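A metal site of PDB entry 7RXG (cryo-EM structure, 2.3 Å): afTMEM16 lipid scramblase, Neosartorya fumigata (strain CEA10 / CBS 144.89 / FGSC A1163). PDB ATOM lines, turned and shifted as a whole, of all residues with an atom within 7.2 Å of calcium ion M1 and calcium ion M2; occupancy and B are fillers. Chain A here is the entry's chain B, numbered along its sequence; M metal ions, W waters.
The side-chain carboxylate (OE2) of Glu 445 lies close to the side-chain amino group (NZ) of Lys 550, at 2.6 Å.
OD2 of Asp 511 is in hydrogen-bond range of OH of Tyr 506 (2.5 Å).
OD2 of Asp 511 is in salt-bridge range of NZ of Lys 550, at 3.4 Å.
OD1 of Asp 547 sits close to NZ of Lys 550.
OE2 of Glu 543 sits close to ND2 of Asn 539 (3.2 Å).
NZ of Lys 550 touches calcium ion M2 (3.9 Å).
Within 4 Å of calcium ion M2: Glu 445, Asp 511, Glu 514, Glu 543, Asp 547 and Lys 550.
Along chain A the residues within 4 Å of calcium ion M2 span positions 445 to 550.
Calcium ion M1 is bound by OE2 of Glu 514 (2.4 Å), water W1 (2.5 Å), OE1 of Glu 445 (2.6 Å), OE2 of Glu 543 (2.7 Å) and OE1 of Glu 543 (2.7 Å).
Calcium ion M1 has five donor atoms within binding distance.
Calcium ion M2 is bound by OE1 of Glu 543, OE2 of Glu 445, OD1 of Asp 511, water W2, OE1 of Glu 514, OD1 of Asp 547 and OD2 of Asp 547.
Water W1 lies within hydrogen-bond range of OD1 of Asn 539 (2.6 Å) and O of Gln 438 (3.0 Å).
Water W2 bridges the side-chain hydroxyl (OH) of Tyr 180 (2.9 Å) and the backbone carbonyl oxygen (O) of Asp 511 (3.0 Å).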
ATOM      1  N   TYR A 180      31.159  -3.747  12.052  1.00  0.00           N
ATOM      2  CA  TYR A 180      30.640  -4.459  13.220  1.00  0.00           C
ATOM      3  C   TYR A 180      31.772  -5.054  14.050  1.00  0.00           C
ATOM      4  O   TYR A 180      31.773  -4.936  15.274  1.00  0.00           O
ATOM      5  CB  TYR A 180      29.663  -5.553  12.826  1.00  0.00           C
ATOM      6  CG  TYR A 180      29.462  -6.550  13.943  1.00  0.00           C
ATOM      7  CD1 TYR A 180      28.846  -6.181  15.129  1.00  0.00           C
ATOM      8  CD2 TYR A 180      29.926  -7.859  13.835  1.00  0.00           C
ATOM      9  CE1 TYR A 180      28.673  -7.069  16.163  1.00  0.00           C
ATOM     10  CE2 TYR A 180      29.754  -8.755  14.857  1.00  0.00           C
ATOM     11  CZ  TYR A 180      29.130  -8.360  16.017  1.00  0.00           C
ATOM     12  OH  TYR A 180      28.958  -9.256  17.040  1.00  0.00           O
ATOM     13  N   LEU A 184      32.842  -4.116  17.832  1.00  0.00           N
ATOM     14  CA  LEU A 184      32.885  -5.125  18.879  1.00  0.00           C
ATOM     15  C   LEU A 184      34.250  -5.161  19.555  1.00  0.00           C
ATOM     16  O   LEU A 184      34.331  -5.266  20.779  1.00  0.00           O
ATOM     17  CB  LEU A 184      32.525  -6.494  18.315  1.00  0.00           C
ATOM     18  CG  LEU A 184      32.420  -7.646  19.318  1.00  0.00           C
ATOM     19  CD1 LEU A 184      31.547  -7.273  20.485  1.00  0.00           C
ATOM     20  CD2 LEU A 184      31.919  -8.899  18.645  1.00  0.00           C
ATOM     21  N   ALA A 437      21.263 -15.195  30.272  1.00  0.00           N
ATOM     22  CA  ALA A 437      20.808 -14.850  28.940  1.00  0.00           C
ATOM     23  C   ALA A 437      21.970 -14.824  27.954  1.00  0.00           C
ATOM     24  O   ALA A 437      21.806 -15.237  26.808  1.00  0.00           O
ATOM     25  CB  ALA A 437      20.079 -13.518  28.946  1.00  0.00           C
ATOM     26  N   GLN A 438      23.150 -14.365  28.387  1.00  0.00           N
ATOM     27  CA  GLN A 438      24.305 -14.369  27.498  1.00  0.00           C
ATOM     28  C   GLN A 438      24.703 -15.792  27.106  1.00  0.00           C
ATOM     29  O   GLN A 438      24.939 -16.066  25.929  1.00  0.00           O
ATOM     30  CB  GLN A 438      25.489 -13.661  28.164  1.00  0.00           C
ATOM     31  CG  GLN A 438      25.178 -12.322  28.762  1.00  0.00           C
ATOM     32  CD  GLN A 438      24.833 -11.281  27.719  1.00  0.00           C
ATOM     33  OE1 GLN A 438      23.715 -10.779  27.674  1.00  0.00           O
ATOM     34  NE2 GLN A 438      25.802 -10.951  26.878  1.00  0.00           N
ATOM     35  N   ILE A 439      24.760 -16.701  28.085  1.00  0.00           N
ATOM     36  CA  ILE A 439      25.145 -18.077  27.780  1.00  0.00           C
ATOM     37  C   ILE A 439      24.088 -18.758  26.911  1.00  0.00           C
ATOM     38  O   ILE A 439      24.414 -19.434  25.927  1.00  0.00           O
ATOM     39  CB  ILE A 439      25.394 -18.850  29.091  1.00  0.00           C
ATOM     40  CG1 ILE A 439      26.534 -18.208  29.878  1.00  0.00           C
ATOM     41  CG2 ILE A 439      25.707 -20.305  28.788  1.00  0.00           C
ATOM     42  CD1 ILE A 439      26.595 -18.627  31.318  1.00  0.00           C
ATOM     43  N   VAL A 440      22.813 -18.594  27.257  1.00  0.00           N
ATOM     44  CA  VAL A 440      21.750 -19.226  26.491  1.00  0.00           C
ATOM     45  C   VAL A 440      21.671 -18.641  25.083  1.00  0.00           C
ATOM     46  O   VAL A 440      21.355 -19.348  24.126  1.00  0.00           O
ATOM     47  CB  VAL A 440      20.405 -19.091  27.233  1.00  0.00           C
ATOM     48  CG1 VAL A 440      19.271 -19.592  26.375  1.00  0.00           C
ATOM     49  CG2 VAL A 440      20.462 -19.846  28.551  1.00  0.00           C
ATOM     50  N   GLY A 441      21.964 -17.345  24.940  1.00  0.00           N
ATOM     51  CA  GLY A 441      21.968 -16.743  23.626  1.00  0.00           C
ATOM     52  C   GLY A 441      23.147 -17.195  22.788  1.00  0.00           C
ATOM     53  O   GLY A 441      22.993 -17.393  21.589  1.00  0.00           O
ATOM     54  N   PHE A 442      24.304 -17.372  23.408  1.00  0.00           N
ATOM     55  CA  PHE A 442      25.424 -17.993  22.702  1.00  0.00           C
ATOM     56  C   PHE A 442      25.038 -19.378  22.191  1.00  0.00           C
ATOM     57  O   PHE A 442      25.305 -19.710  21.029  1.00  0.00           O
ATOM     58  CB  PHE A 442      26.639 -18.093  23.624  1.00  0.00           C
ATOM     59  CG  PHE A 442      27.701 -19.036  23.145  1.00  0.00           C
ATOM     60  CD1 PHE A 442      28.600 -18.643  22.165  1.00  0.00           C
ATOM     61  CD2 PHE A 442      27.800 -20.310  23.672  1.00  0.00           C
ATOM     62  CE1 PHE A 442      29.574 -19.515  21.721  1.00  0.00           C
ATOM     63  CE2 PHE A 442      28.779 -21.181  23.219  1.00  0.00           C
ATOM     64  CZ  PHE A 442      29.666 -20.775  22.255  1.00  0.00           C
ATOM     65  N   ALA A 443      24.388 -20.169  23.041  1.00  0.00           N
ATOM     66  CA  ALA A 443      23.921 -21.492  22.614  1.00  0.00           C
ATOM     67  C   ALA A 443      22.973 -21.384  21.430  1.00  0.00           C
ATOM     68  O   ALA A 443      23.256 -21.896  20.348  1.00  0.00           O
ATOM     69  CB  ALA A 443      23.257 -22.220  23.781  1.00  0.00           C
ATOM     70  N   GLU A 445      22.469 -19.117  19.376  1.00  0.00           N
ATOM     71  CA  GLU A 445      22.996 -18.373  18.237  1.00  0.00           C
ATOM     72  C   GLU A 445      24.014 -19.180  17.442  1.00  0.00           C
ATOM     73  O   GLU A 445      23.986 -19.138  16.210  1.00  0.00           O
ATOM     74  CB  GLU A 445      23.621 -17.071  18.718  1.00  0.00           C
ATOM     75  CG  GLU A 445      24.081 -16.149  17.618  1.00  0.00           C
ATOM     76  CD  GLU A 445      24.584 -14.825  18.157  1.00  0.00           C
ATOM     77  OE1 GLU A 445      24.730 -14.691  19.382  1.00  0.00           O
ATOM     78  OE2 GLU A 445      24.829 -13.912  17.348  1.00  0.00           O
ATOM     79  N   THR A 446      24.921 -19.892  18.104  1.00  0.00           N
ATOM     80  CA  THR A 446      25.940 -20.650  17.403  1.00  0.00           C
ATOM     81  C   THR A 446      25.685 -22.152  17.397  1.00  0.00           C
ATOM     82  O   THR A 446      25.803 -22.775  16.344  1.00  0.00           O
ATOM     83  CB  THR A 446      27.324 -20.383  18.000  1.00  0.00           C
ATOM     84  OG1 THR A 446      27.353 -20.829  19.363  1.00  0.00           O
ATOM     85  CG2 THR A 446      27.661 -18.912  17.936  1.00  0.00           C
ATOM     86  N   TYR A 506      23.299 -14.072   6.495  1.00  0.00           N
ATOM     87  CA  TYR A 506      23.805 -13.285   7.609  1.00  0.00           C
ATOM     88  C   TYR A 506      23.350 -11.837   7.510  1.00  0.00           C
ATOM     89  O   TYR A 506      23.465 -11.209   6.455  1.00  0.00           O
ATOM     90  CB  TYR A 506      25.333 -13.346   7.663  1.00  0.00           C
ATOM     91  CG  TYR A 506      25.911 -12.529   8.785  1.00  0.00           C
ATOM     92  CD1 TYR A 506      25.759 -12.922  10.105  1.00  0.00           C
ATOM     93  CD2 TYR A 506      26.594 -11.347   8.534  1.00  0.00           C
ATOM     94  CE1 TYR A 506      26.282 -12.174  11.135  1.00  0.00           C
ATOM     95  CE2 TYR A 506      27.126 -10.590   9.558  1.00  0.00           C
ATOM     96  CZ  TYR A 506      26.961 -11.016  10.859  1.00  0.00           C
ATOM     97  OH  TYR A 506      27.484 -10.268  11.888  1.00  0.00           O
ATOM     98  N   ASP A 510      21.602  -7.911  13.195  1.00  0.00           N
ATOM     99  CA  ASP A 510      21.256  -8.718  14.365  1.00  0.00           C
ATOM    100  C   ASP A 510      22.356  -8.681  15.411  1.00  0.00           C
ATOM    101  O   ASP A 510      22.091  -8.527  16.602  1.00  0.00           O
ATOM    102  CB  ASP A 510      20.967 -10.154  13.953  1.00  0.00           C
ATOM    103  CG  ASP A 510      19.916 -10.250  12.862  1.00  0.00           C
ATOM    104  OD1 ASP A 510      18.964  -9.447  12.890  1.00  0.00           O
ATOM    105  OD2 ASP A 510      20.044 -11.119  11.986  1.00  0.00           O
ATOM    106  N   ASP A 511      23.613  -8.804  14.977  1.00  0.00           N
ATOM    107  CA  ASP A 511      24.721  -8.781  15.913  1.00  0.00           C
ATOM    108  C   ASP A 511      24.893  -7.397  16.522  1.00  0.00           C
ATOM    109  O   ASP A 511      25.178  -7.259  17.722  1.00  0.00           O
ATOM    110  CB  ASP A 511      26.001  -9.244  15.224  1.00  0.00           C
ATOM    111  CG  ASP A 511      26.017 -10.742  14.992  1.00  0.00           C
ATOM    112  OD1 ASP A 511      25.247 -11.449  15.651  1.00  0.00           O
ATOM    113  OD2 ASP A 511      26.808 -11.209  14.153  1.00  0.00           O
ATOM    114  N   LEU A 512      24.721  -6.355  15.714  1.00  0.00           N
ATOM    115  CA  LEU A 512      24.766  -4.996  16.249  1.00  0.00           C
ATOM    116  C   LEU A 512      23.656  -4.763  17.266  1.00  0.00           C
ATOM    117  O   LEU A 512      23.880  -4.142  18.305  1.00  0.00           O
ATOM    118  CB  LEU A 512      24.699  -3.969  15.121  1.00  0.00           C
ATOM    119  CG  LEU A 512      25.992  -3.777  14.342  1.00  0.00           C
ATOM    120  CD1 LEU A 512      25.695  -3.140  12.986  1.00  0.00           C
ATOM    121  CD2 LEU A 512      26.975  -2.943  15.130  1.00  0.00           C
ATOM    122  N   GLU A 514      22.241  -7.052  19.155  1.00  0.00           N
ATOM    123  CA  GLU A 514      22.588  -7.775  20.375  1.00  0.00           C
ATOM    124  C   GLU A 514      23.604  -6.996  21.201  1.00  0.00           C
ATOM    125  O   GLU A 514      23.432  -6.843  22.421  1.00  0.00           O
ATOM    126  CB  GLU A 514      23.125  -9.158  20.028  1.00  0.00           C
ATOM    127  CG  GLU A 514      23.545  -9.961  21.228  1.00  0.00           C
ATOM    128  CD  GLU A 514      24.289 -11.229  20.877  1.00  0.00           C
ATOM    129  OE1 GLU A 514      24.199 -11.664  19.715  1.00  0.00           O
ATOM    130  OE2 GLU A 514      24.959 -11.785  21.770  1.00  0.00           O
ATOM    131  N   MET A 515      24.652  -6.483  20.563  1.00  0.00           N
ATOM    132  CA  MET A 515      25.660  -5.734  21.315  1.00  0.00           C
ATOM    133  C   MET A 515      25.103  -4.447  21.898  1.00  0.00           C
ATOM    134  O   MET A 515      25.460  -4.067  23.013  1.00  0.00           O
ATOM    135  CB  MET A 515      26.875  -5.450  20.428  1.00  0.00           C
ATOM    136  CG  MET A 515      27.748  -6.674  20.198  1.00  0.00           C
ATOM    137  SD  MET A 515      28.328  -7.442  21.730  1.00  0.00           S
ATOM    138  CE  MET A 515      27.190  -8.806  21.877  1.00  0.00           C
ATOM    139  N   GLN A 518      22.979  -5.287  24.925  1.00  0.00           N
ATOM    140  CA  GLN A 518      23.881  -5.591  26.029  1.00  0.00           C
ATOM    141  C   GLN A 518      24.433  -4.315  26.662  1.00  0.00           C
ATOM    142  O   GLN A 518      24.472  -4.175  27.897  1.00  0.00           O
ATOM    143  CB  GLN A 518      25.002  -6.487  25.528  1.00  0.00           C
ATOM    144  CG  GLN A 518      25.905  -7.018  26.599  1.00  0.00           C
ATOM    145  CD  GLN A 518      27.268  -7.394  26.075  1.00  0.00           C
ATOM    146  OE1 GLN A 518      28.120  -6.541  25.893  1.00  0.00           O
ATOM    147  NE2 GLN A 518      27.469  -8.674  25.819  1.00  0.00           N
ATOM    148  N   ASN A 539      32.010 -12.319  27.708  1.00  0.00           N
ATOM    149  CA  ASN A 539      31.103 -12.679  26.640  1.00  0.00           C
ATOM    150  C   ASN A 539      31.514 -12.044  25.316  1.00  0.00           C
ATOM    151  O   ASN A 539      31.334 -12.650  24.267  1.00  0.00           O
ATOM    152  CB  ASN A 539      29.672 -12.273  26.978  1.00  0.00           C
ATOM    153  CG  ASN A 539      28.707 -12.528  25.836  1.00  0.00           C
ATOM    154  OD1 ASN A 539      28.184 -13.624  25.698  1.00  0.00           O
ATOM    155  ND2 ASN A 539      28.480 -11.519  25.008  1.00  0.00           N
ATOM    156  N   GLU A 543      32.412 -13.422  21.887  1.00  0.00           N
ATOM    157  CA  GLU A 543      31.453 -13.022  20.871  1.00  0.00           C
ATOM    158  C   GLU A 543      32.128 -12.722  19.553  1.00  0.00           C
ATOM    159  O   GLU A 543      31.596 -13.062  18.491  1.00  0.00           O
ATOM    160  CB  GLU A 543      30.665 -11.798  21.344  1.00  0.00           C
ATOM    161  CG  GLU A 543      29.459 -11.458  20.507  1.00  0.00           C
ATOM    162  CD  GLU A 543      28.265 -12.313  20.852  1.00  0.00           C
ATOM    163  OE1 GLU A 543      27.449 -12.599  19.942  1.00  0.00           O
ATOM    164  OE2 GLU A 543      28.126 -12.707  22.019  1.00  0.00           O
ATOM    165  N   SER A 546      32.987 -16.231  18.119  1.00  0.00           N
ATOM    166  CA  SER A 546      31.807 -17.022  17.786  1.00  0.00           C
ATOM    167  C   SER A 546      30.982 -16.399  16.671  1.00  0.00           C
ATOM    168  O   SER A 546      30.396 -17.122  15.871  1.00  0.00           O
ATOM    169  CB  SER A 546      30.963 -17.245  19.046  1.00  0.00           C
ATOM    170  OG  SER A 546      30.071 -16.171  19.259  1.00  0.00           O
ATOM    171  N   ASP A 547      30.960 -15.070  16.582  1.00  0.00           N
ATOM    172  CA  ASP A 547      30.272 -14.425  15.465  1.00  0.00           C
ATOM    173  C   ASP A 547      31.027 -14.637  14.158  1.00  0.00           C
ATOM    174  O   ASP A 547      30.414 -14.855  13.113  1.00  0.00           O
ATOM    175  CB  ASP A 547      30.075 -12.940  15.743  1.00  0.00           C
ATOM    176  CG  ASP A 547      28.845 -12.659  16.568  1.00  0.00           C
ATOM    177  OD1 ASP A 547      27.986 -13.549  16.663  1.00  0.00           O
ATOM    178  OD2 ASP A 547      28.748 -11.553  17.127  1.00  0.00           O
ATOM    179  N   LYS A 550      30.197 -18.111  13.164  1.00  0.00           N
ATOM    180  CA  LYS A 550      28.845 -18.179  12.628  1.00  0.00           C
ATOM    181  C   LYS A 550      28.795 -17.662  11.199  1.00  0.00           C
ATOM    182  O   LYS A 550      28.119 -18.234  10.344  1.00  0.00           O
ATOM    183  CB  LYS A 550      27.891 -17.380  13.517  1.00  0.00           C
ATOM    184  CG  LYS A 550      26.496 -17.240  12.966  1.00  0.00           C
ATOM    185  CD  LYS A 550      25.638 -16.417  13.910  1.00  0.00           C
ATOM    186  CE  LYS A 550      26.072 -14.970  13.934  1.00  0.00           C
ATOM    187  NZ  LYS A 550      25.213 -14.145  14.808  1.00  0.00           N
HETATM  188 CA    CA M   1      25.843 -14.010  21.592  1.00  0.00          CA
HETATM  189 CA    CA M   2      26.178 -12.035  17.988  1.00  0.00          CA
HETATM  190  O   HOH W   1      26.255 -14.143  24.082  1.00  0.00           O
HETATM  191  O   HOH W   2      26.721  -9.597  18.784  1.00  0.00           O
